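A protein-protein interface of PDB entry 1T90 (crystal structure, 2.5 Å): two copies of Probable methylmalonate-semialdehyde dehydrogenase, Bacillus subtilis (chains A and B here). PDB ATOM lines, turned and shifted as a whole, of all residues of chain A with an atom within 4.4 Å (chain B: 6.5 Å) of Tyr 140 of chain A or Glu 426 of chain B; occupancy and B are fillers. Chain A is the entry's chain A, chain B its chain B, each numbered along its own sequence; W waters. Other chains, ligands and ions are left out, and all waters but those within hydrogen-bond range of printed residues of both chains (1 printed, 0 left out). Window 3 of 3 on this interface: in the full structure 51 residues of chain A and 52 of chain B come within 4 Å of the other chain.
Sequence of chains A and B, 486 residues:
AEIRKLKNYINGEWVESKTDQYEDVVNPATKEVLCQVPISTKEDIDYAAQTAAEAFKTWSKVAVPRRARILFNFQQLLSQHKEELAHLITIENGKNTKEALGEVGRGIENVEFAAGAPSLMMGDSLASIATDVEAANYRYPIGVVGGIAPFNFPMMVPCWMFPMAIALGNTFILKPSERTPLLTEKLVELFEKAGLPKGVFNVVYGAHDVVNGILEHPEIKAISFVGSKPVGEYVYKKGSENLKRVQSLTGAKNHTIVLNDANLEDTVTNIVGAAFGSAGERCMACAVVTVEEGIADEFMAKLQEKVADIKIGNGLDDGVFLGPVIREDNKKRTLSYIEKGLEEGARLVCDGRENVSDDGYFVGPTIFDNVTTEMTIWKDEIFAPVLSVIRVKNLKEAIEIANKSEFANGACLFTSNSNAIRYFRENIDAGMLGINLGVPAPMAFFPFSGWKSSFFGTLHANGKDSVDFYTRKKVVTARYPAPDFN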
ATOM      1  N   TYR A 138      13.999   9.374  -2.972  1.00  0.00           N
ATOM      2  CA  TYR A 138      13.732   9.639  -1.569  1.00  0.00           C
ATOM      3  C   TYR A 138      13.826  11.121  -1.276  1.00  0.00           C
ATOM      4  O   TYR A 138      14.408  11.885  -2.051  1.00  0.00           O
ATOM      5  CB  TYR A 138      14.753   8.914  -0.686  1.00  0.00           C
ATOM      6  CG  TYR A 138      14.895   7.438  -0.971  1.00  0.00           C
ATOM      7  CD1 TYR A 138      15.575   6.987  -2.102  1.00  0.00           C
ATOM      8  CD2 TYR A 138      14.330   6.489  -0.120  1.00  0.00           C
ATOM      9  CE1 TYR A 138      15.685   5.627  -2.378  1.00  0.00           C
ATOM     10  CE2 TYR A 138      14.433   5.129  -0.391  1.00  0.00           C
ATOM     11  CZ  TYR A 138      15.112   4.709  -1.523  1.00  0.00           C
ATOM     12  OH  TYR A 138      15.201   3.366  -1.796  1.00  0.00           O
ATOM     13  N   ARG A 139      13.249  11.520  -0.150  1.00  0.00           N
ATOM     14  CA  ARG A 139      13.289  12.907   0.264  1.00  0.00           C
ATOM     15  C   ARG A 139      14.194  13.034   1.471  1.00  0.00           C
ATOM     16  O   ARG A 139      14.182  12.185   2.377  1.00  0.00           O
ATOM     17  CB  ARG A 139      11.897  13.417   0.623  1.00  0.00           C
ATOM     18  CG  ARG A 139      10.992  13.640  -0.561  1.00  0.00           C
ATOM     19  CD  ARG A 139       9.612  14.039  -0.079  1.00  0.00           C
ATOM     20  NE  ARG A 139       8.606  13.865  -1.119  1.00  0.00           N
ATOM     21  CZ  ARG A 139       8.156  14.855  -1.874  1.00  0.00           C
ATOM     22  NH1 ARG A 139       8.624  16.083  -1.686  1.00  0.00           N
ATOM     23  NH2 ARG A 139       7.250  14.618  -2.815  1.00  0.00           N
ATOM     24  N   TYR A 140      14.985  14.101   1.462  1.00  0.00           N
ATOM     25  CA  TYR A 140      15.911  14.397   2.541  1.00  0.00           C
ATOM     26  C   TYR A 140      15.750  15.852   2.914  1.00  0.00           C
ATOM     27  O   TYR A 140      15.302  16.668   2.100  1.00  0.00           O
ATOM     28  CB  TYR A 140      17.364  14.178   2.096  1.00  0.00           C
ATOM     29  CG  TYR A 140      17.731  12.743   1.805  1.00  0.00           C
ATOM     30  CD1 TYR A 140      17.376  12.137   0.598  1.00  0.00           C
ATOM     31  CD2 TYR A 140      18.412  11.985   2.745  1.00  0.00           C
ATOM     32  CE1 TYR A 140      17.697  10.800   0.342  1.00  0.00           C
ATOM     33  CE2 TYR A 140      18.733  10.656   2.506  1.00  0.00           C
ATOM     34  CZ  TYR A 140      18.374  10.069   1.311  1.00  0.00           C
ATOM     35  OH  TYR A 140      18.682   8.749   1.102  1.00  0.00           O
ATOM     36  N   PRO A 141      16.096  16.201   4.160  1.00  0.00           N
ATOM     37  CA  PRO A 141      15.977  17.602   4.562  1.00  0.00           C
ATOM     38  C   PRO A 141      17.122  18.330   3.858  1.00  0.00           C
ATOM     39  O   PRO A 141      18.107  17.709   3.477  1.00  0.00           O
ATOM     40  CB  PRO A 141      16.160  17.541   6.073  1.00  0.00           C
ATOM     41  CG  PRO A 141      17.094  16.378   6.254  1.00  0.00           C
ATOM     42  CD  PRO A 141      16.524  15.357   5.289  1.00  0.00           C
ATOM     43  N   ILE A 142      16.996  19.632   3.672  1.00  0.00           N
ATOM     44  CA  ILE A 142      18.046  20.374   3.004  1.00  0.00           C
ATOM     45  C   ILE A 142      19.138  20.883   3.947  1.00  0.00           C
ATOM     46  O   ILE A 142      20.289  21.022   3.545  1.00  0.00           O
ATOM     47  CB  ILE A 142      17.447  21.555   2.199  1.00  0.00           C
ATOM     48  CG1 ILE A 142      16.494  22.360   3.079  1.00  0.00           C
ATOM     49  CG2 ILE A 142      16.683  21.029   0.989  1.00  0.00           C
ATOM     50  CD1 ILE A 142      15.699  23.415   2.322  1.00  0.00           C
ATOM     51  N   THR A 471      12.506  20.289   1.398  1.00  0.00           N
ATOM     52  CA  THR A 471      13.131  18.999   1.209  1.00  0.00           C
ATOM     53  C   THR A 471      13.688  18.858  -0.207  1.00  0.00           C
ATOM     54  O   THR A 471      13.251  19.557  -1.119  1.00  0.00           O
ATOM     55  CB  THR A 471      12.070  17.897   1.493  1.00  0.00           C
ATOM     56  OG1 THR A 471      12.708  16.706   1.945  1.00  0.00           O
ATOM     57  CG2 THR A 471      11.272  17.590   0.249  1.00  0.00           C
ATOM     58  N   ARG A 472      14.663  17.973  -0.389  1.00  0.00           N
ATOM     59  CA  ARG A 472      15.219  17.743  -1.721  1.00  0.00           C
ATOM     60  C   ARG A 472      15.226  16.233  -2.006  1.00  0.00           C
ATOM     61  O   ARG A 472      15.146  15.414  -1.079  1.00  0.00           O
ATOM     62  CB  ARG A 472      16.623  18.342  -1.836  1.00  0.00           C
ATOM     63  CG  ARG A 472      17.717  17.634  -1.047  1.00  0.00           C
ATOM     64  CD  ARG A 472      18.622  16.898  -2.011  1.00  0.00           C
ATOM     65  NE  ARG A 472      19.954  16.717  -1.463  1.00  0.00           N
ATOM     66  CZ  ARG A 472      20.981  16.232  -2.152  1.00  0.00           C
ATOM     67  NH1 ARG A 472      22.165  16.098  -1.565  1.00  0.00           N
ATOM     68  NH2 ARG A 472      20.822  15.883  -3.423  1.00  0.00           N
ATOM     69  N   LYS A 474      16.663  12.517  -3.940  1.00  0.00           N
ATOM     70  CA  LYS A 474      17.778  11.744  -4.455  1.00  0.00           C
ATOM     71  C   LYS A 474      17.134  10.528  -5.086  1.00  0.00           C
ATOM     72  O   LYS A 474      16.353   9.834  -4.445  1.00  0.00           O
ATOM     73  CB  LYS A 474      18.725  11.301  -3.343  1.00  0.00           C
ATOM     74  CG  LYS A 474      19.580  12.408  -2.781  1.00  0.00           C
ATOM     75  CD  LYS A 474      20.787  11.834  -2.056  1.00  0.00           C
ATOM     76  CE  LYS A 474      20.862  12.299  -0.601  1.00  0.00           C
ATOM     77  NZ  LYS A 474      22.182  11.941   0.020  1.00  0.00           N
ATOM     78  N   ILE B 421      26.137   0.478  -0.379  1.00  0.00           N
ATOM     79  CA  ILE B 421      25.118   1.166  -1.149  1.00  0.00           C
ATOM     80  C   ILE B 421      24.329   2.169  -0.302  1.00  0.00           C
ATOM     81  O   ILE B 421      24.210   3.335  -0.669  1.00  0.00           O
ATOM     82  CB  ILE B 421      24.174   0.145  -1.806  1.00  0.00           C
ATOM     83  CG1 ILE B 421      24.995  -0.754  -2.732  1.00  0.00           C
ATOM     84  CG2 ILE B 421      23.078   0.855  -2.588  1.00  0.00           C
ATOM     85  CD1 ILE B 421      24.225  -1.878  -3.367  1.00  0.00           C
ATOM     86  N   ARG B 422      23.799   1.729   0.835  1.00  0.00           N
ATOM     87  CA  ARG B 422      23.046   2.633   1.697  1.00  0.00           C
ATOM     88  C   ARG B 422      23.921   3.806   2.131  1.00  0.00           C
ATOM     89  O   ARG B 422      23.515   4.967   2.037  1.00  0.00           O
ATOM     90  CB  ARG B 422      22.530   1.913   2.953  1.00  0.00           C
ATOM     91  CG  ARG B 422      21.864   2.869   3.936  1.00  0.00           C
ATOM     92  CD  ARG B 422      21.444   2.204   5.236  1.00  0.00           C
ATOM     93  NE  ARG B 422      20.993   3.205   6.202  1.00  0.00           N
ATOM     94  CZ  ARG B 422      19.799   3.794   6.187  1.00  0.00           C
ATOM     95  NH1 ARG B 422      19.495   4.703   7.100  1.00  0.00           N
ATOM     96  NH2 ARG B 422      18.894   3.455   5.281  1.00  0.00           N
ATOM     97  N   TYR B 423      25.119   3.489   2.618  1.00  0.00           N
ATOM     98  CA  TYR B 423      26.052   4.502   3.083  1.00  0.00           C
ATOM     99  C   TYR B 423      26.268   5.547   1.991  1.00  0.00           C
ATOM    100  O   TYR B 423      26.266   6.753   2.256  1.00  0.00           O
ATOM    101  CB  TYR B 423      27.389   3.857   3.455  1.00  0.00           C
ATOM    102  CG  TYR B 423      28.349   4.826   4.089  1.00  0.00           C
ATOM    103  CD1 TYR B 423      28.266   5.124   5.449  1.00  0.00           C
ATOM    104  CD2 TYR B 423      29.306   5.491   3.322  1.00  0.00           C
ATOM    105  CE1 TYR B 423      29.112   6.066   6.034  1.00  0.00           C
ATOM    106  CE2 TYR B 423      30.157   6.436   3.893  1.00  0.00           C
ATOM    107  CZ  TYR B 423      30.053   6.719   5.253  1.00  0.00           C
ATOM    108  OH  TYR B 423      30.884   7.653   5.826  1.00  0.00           O
ATOM    109  N   PHE B 424      26.459   5.063   0.765  1.00  0.00           N
ATOM    110  CA  PHE B 424      26.668   5.915  -0.398  1.00  0.00           C
ATOM    111  C   PHE B 424      25.494   6.874  -0.568  1.00  0.00           C
ATOM    112  O   PHE B 424      25.669   8.093  -0.611  1.00  0.00           O
ATOM    113  CB  PHE B 424      26.803   5.033  -1.646  1.00  0.00           C
ATOM    114  CG  PHE B 424      26.794   5.790  -2.950  1.00  0.00           C
ATOM    115  CD1 PHE B 424      27.757   6.755  -3.222  1.00  0.00           C
ATOM    116  CD2 PHE B 424      25.845   5.500  -3.924  1.00  0.00           C
ATOM    117  CE1 PHE B 424      27.780   7.419  -4.448  1.00  0.00           C
ATOM    118  CE2 PHE B 424      25.854   6.156  -5.159  1.00  0.00           C
ATOM    119  CZ  PHE B 424      26.827   7.118  -5.422  1.00  0.00           C
ATOM    120  N   ARG B 425      24.291   6.316  -0.654  1.00  0.00           N
ATOM    121  CA  ARG B 425      23.088   7.118  -0.844  1.00  0.00           C
ATOM    122  C   ARG B 425      22.814   8.124   0.272  1.00  0.00           C
ATOM    123  O   ARG B 425      22.350   9.230   0.014  1.00  0.00           O
ATOM    124  CB  ARG B 425      21.866   6.206  -1.010  1.00  0.00           C
ATOM    125  CG  ARG B 425      20.610   6.936  -1.487  1.00  0.00           C
ATOM    126  CD  ARG B 425      19.442   6.685  -0.560  1.00  0.00           C
ATOM    127  NE  ARG B 425      19.124   5.268  -0.480  1.00  0.00           N
ATOM    128  CZ  ARG B 425      18.756   4.640   0.632  1.00  0.00           C
ATOM    129  NH1 ARG B 425      18.652   5.299   1.777  1.00  0.00           N
ATOM    130  NH2 ARG B 425      18.497   3.345   0.590  1.00  0.00           N
ATOM    131  N   GLU B 426      23.098   7.753   1.511  1.00  0.00           N
ATOM    132  CA  GLU B 426      22.830   8.664   2.618  1.00  0.00           C
ATOM    133  C   GLU B 426      23.802   9.823   2.716  1.00  0.00           C
ATOM    134  O   GLU B 426      23.405  10.930   3.085  1.00  0.00           O
ATOM    135  CB  GLU B 426      22.824   7.905   3.951  1.00  0.00           C
ATOM    136  CG  GLU B 426      21.662   6.948   4.114  1.00  0.00           C
ATOM    137  CD  GLU B 426      20.328   7.660   4.096  1.00  0.00           C
ATOM    138  OE1 GLU B 426      20.091   8.494   5.006  1.00  0.00           O
ATOM    139  OE2 GLU B 426      19.522   7.392   3.173  1.00  0.00           O
ATOM    140  N   ASN B 427      25.063   9.579   2.363  1.00  0.00           N
ATOM    141  CA  ASN B 427      26.097  10.604   2.472  1.00  0.00           C
ATOM    142  C   ASN B 427      26.525  11.373   1.221  1.00  0.00           C
ATOM    143  O   ASN B 427      27.105  12.451   1.336  1.00  0.00           O
ATOM    144  CB  ASN B 427      27.339  10.000   3.144  1.00  0.00           C
ATOM    145  CG  ASN B 427      27.038   9.445   4.524  1.00  0.00           C
ATOM    146  OD1 ASN B 427      26.781   8.252   4.691  1.00  0.00           O
ATOM    147  ND2 ASN B 427      27.045  10.315   5.518  1.00  0.00           N
ATOM    148  N   ILE B 428      26.246  10.841   0.035  1.00  0.00           N
ATOM    149  CA  ILE B 428      26.630  11.508  -1.213  1.00  0.00           C
ATOM    150  C   ILE B 428      25.815  12.790  -1.442  1.00  0.00           C
ATOM    151  O   ILE B 428      24.636  12.868  -1.074  1.00  0.00           O
ATOM    152  CB  ILE B 428      26.447  10.545  -2.424  1.00  0.00           C
ATOM    153  CG1 ILE B 428      27.096  11.133  -3.678  1.00  0.00           C
ATOM    154  CG2 ILE B 428      24.974  10.293  -2.677  1.00  0.00           C
ATOM    155  CD1 ILE B 428      28.612  11.103  -3.658  1.00  0.00           C
ATOM    156  N   LEU B 433      21.714   9.171  -8.555  1.00  0.00           N
ATOM    157  CA  LEU B 433      22.626   8.087  -8.247  1.00  0.00           C
ATOM    158  C   LEU B 433      22.406   6.805  -9.027  1.00  0.00           C
ATOM    159  O   LEU B 433      21.271   6.431  -9.348  1.00  0.00           O
ATOM    160  CB  LEU B 433      22.525   7.776  -6.750  1.00  0.00           C
ATOM    161  CG  LEU B 433      23.187   8.701  -5.720  1.00  0.00           C
ATOM    162  CD1 LEU B 433      23.283  10.137  -6.230  1.00  0.00           C
ATOM    163  CD2 LEU B 433      22.393   8.615  -4.425  1.00  0.00           C
HETATM  164  O   HOH W   1      22.693  13.793   2.060  1.00  0.00           O
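Of the 8 printed residues of chain A, 3 touch a printed residue of chain B.
Printed residues of chain B that touch a printed residue of chain A: Arg 425, Glu 426 and Ile 428.
Among the printed residues, no Asp or Glu carboxylate lies within 4 Å of a Lys or Arg side-chain nitrogen of the other chain.
No position is printed for both chains.
Of the 6 pairs that touch across the chains among the printed residues, none has its exchanged pair printed and touching as well.
The side-chain hydroxyl (OH) of Tyr 140 of chain A is in hydrogen-bond range of the side-chain carboxylate (OE2) of Glu 426 of chain B, 2.6 Å away.
The backbone carbonyl oxygen (O) of Glu 426 of chain B sits at hydrogen-bond distance from the side-chain amino group (NZ) of Lys 474 of chain A (3.5 Å).
The side-chain amino group of Lys 474 of chain A lies within hydrogen-bond range of the backbone carbonyl oxygen of Ile 428 of chain B (2.8 Å).
O of Arg 425 of chain B lies within hydrogen-bond range of NZ of Lys 474 of chain A.
The guanidinium group of Arg 425 of chain B lies within salt-bridge range of the side-chain carboxylate of Glu 426 of chain B, at 2.7 Å.
O of Arg 472 of chain A is in hydrogen-bond range of N of Tyr 140 of chain A.
N of Tyr 138 of chain A sits at hydrogen-bond distance from O of Lys 474 of chain A, at 2.8 Å.
The backbone carbonyl oxygen (O) of Tyr 140 of chain A sits at hydrogen-bond distance from the side-chain hydroxyl (OG1) of Thr 471 of chain A, 2.6 Å away.
Among the printed residues, pairs that only touch across the chains: Tyr 138 of chain A with Arg 425 of chain B (3.9 Å) and Tyr 140 of chain A with Arg 425 of chain B (2.8 Å).
Of chain B, only Arg 425 and Glu 426 come within 4 Å of Tyr 140 of chain A.
Printed residues of chain B within 4 Å of Lys 474 of chain A: Arg 425, Glu 426 and Ile 428.
Printed residues of chain A within 4 Å of Arg 425 of chain B: Tyr 138 (3.9 Å), Tyr 140 (2.8 Å) and Lys 474 (2.7 Å).
Printed residues of chain A within 4 Å of Ile 428 of chain B: Lys 474.
The nearest printed residue of chain A that does not touch Arg 425 of chain B is Arg 472 of chain A (7.0 Å).
Water W1 lies within hydrogen-bond range of NZ of Lys 474 of chain A (2.8 Å) and O of Glu 426 of chain B (3.1 Å).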
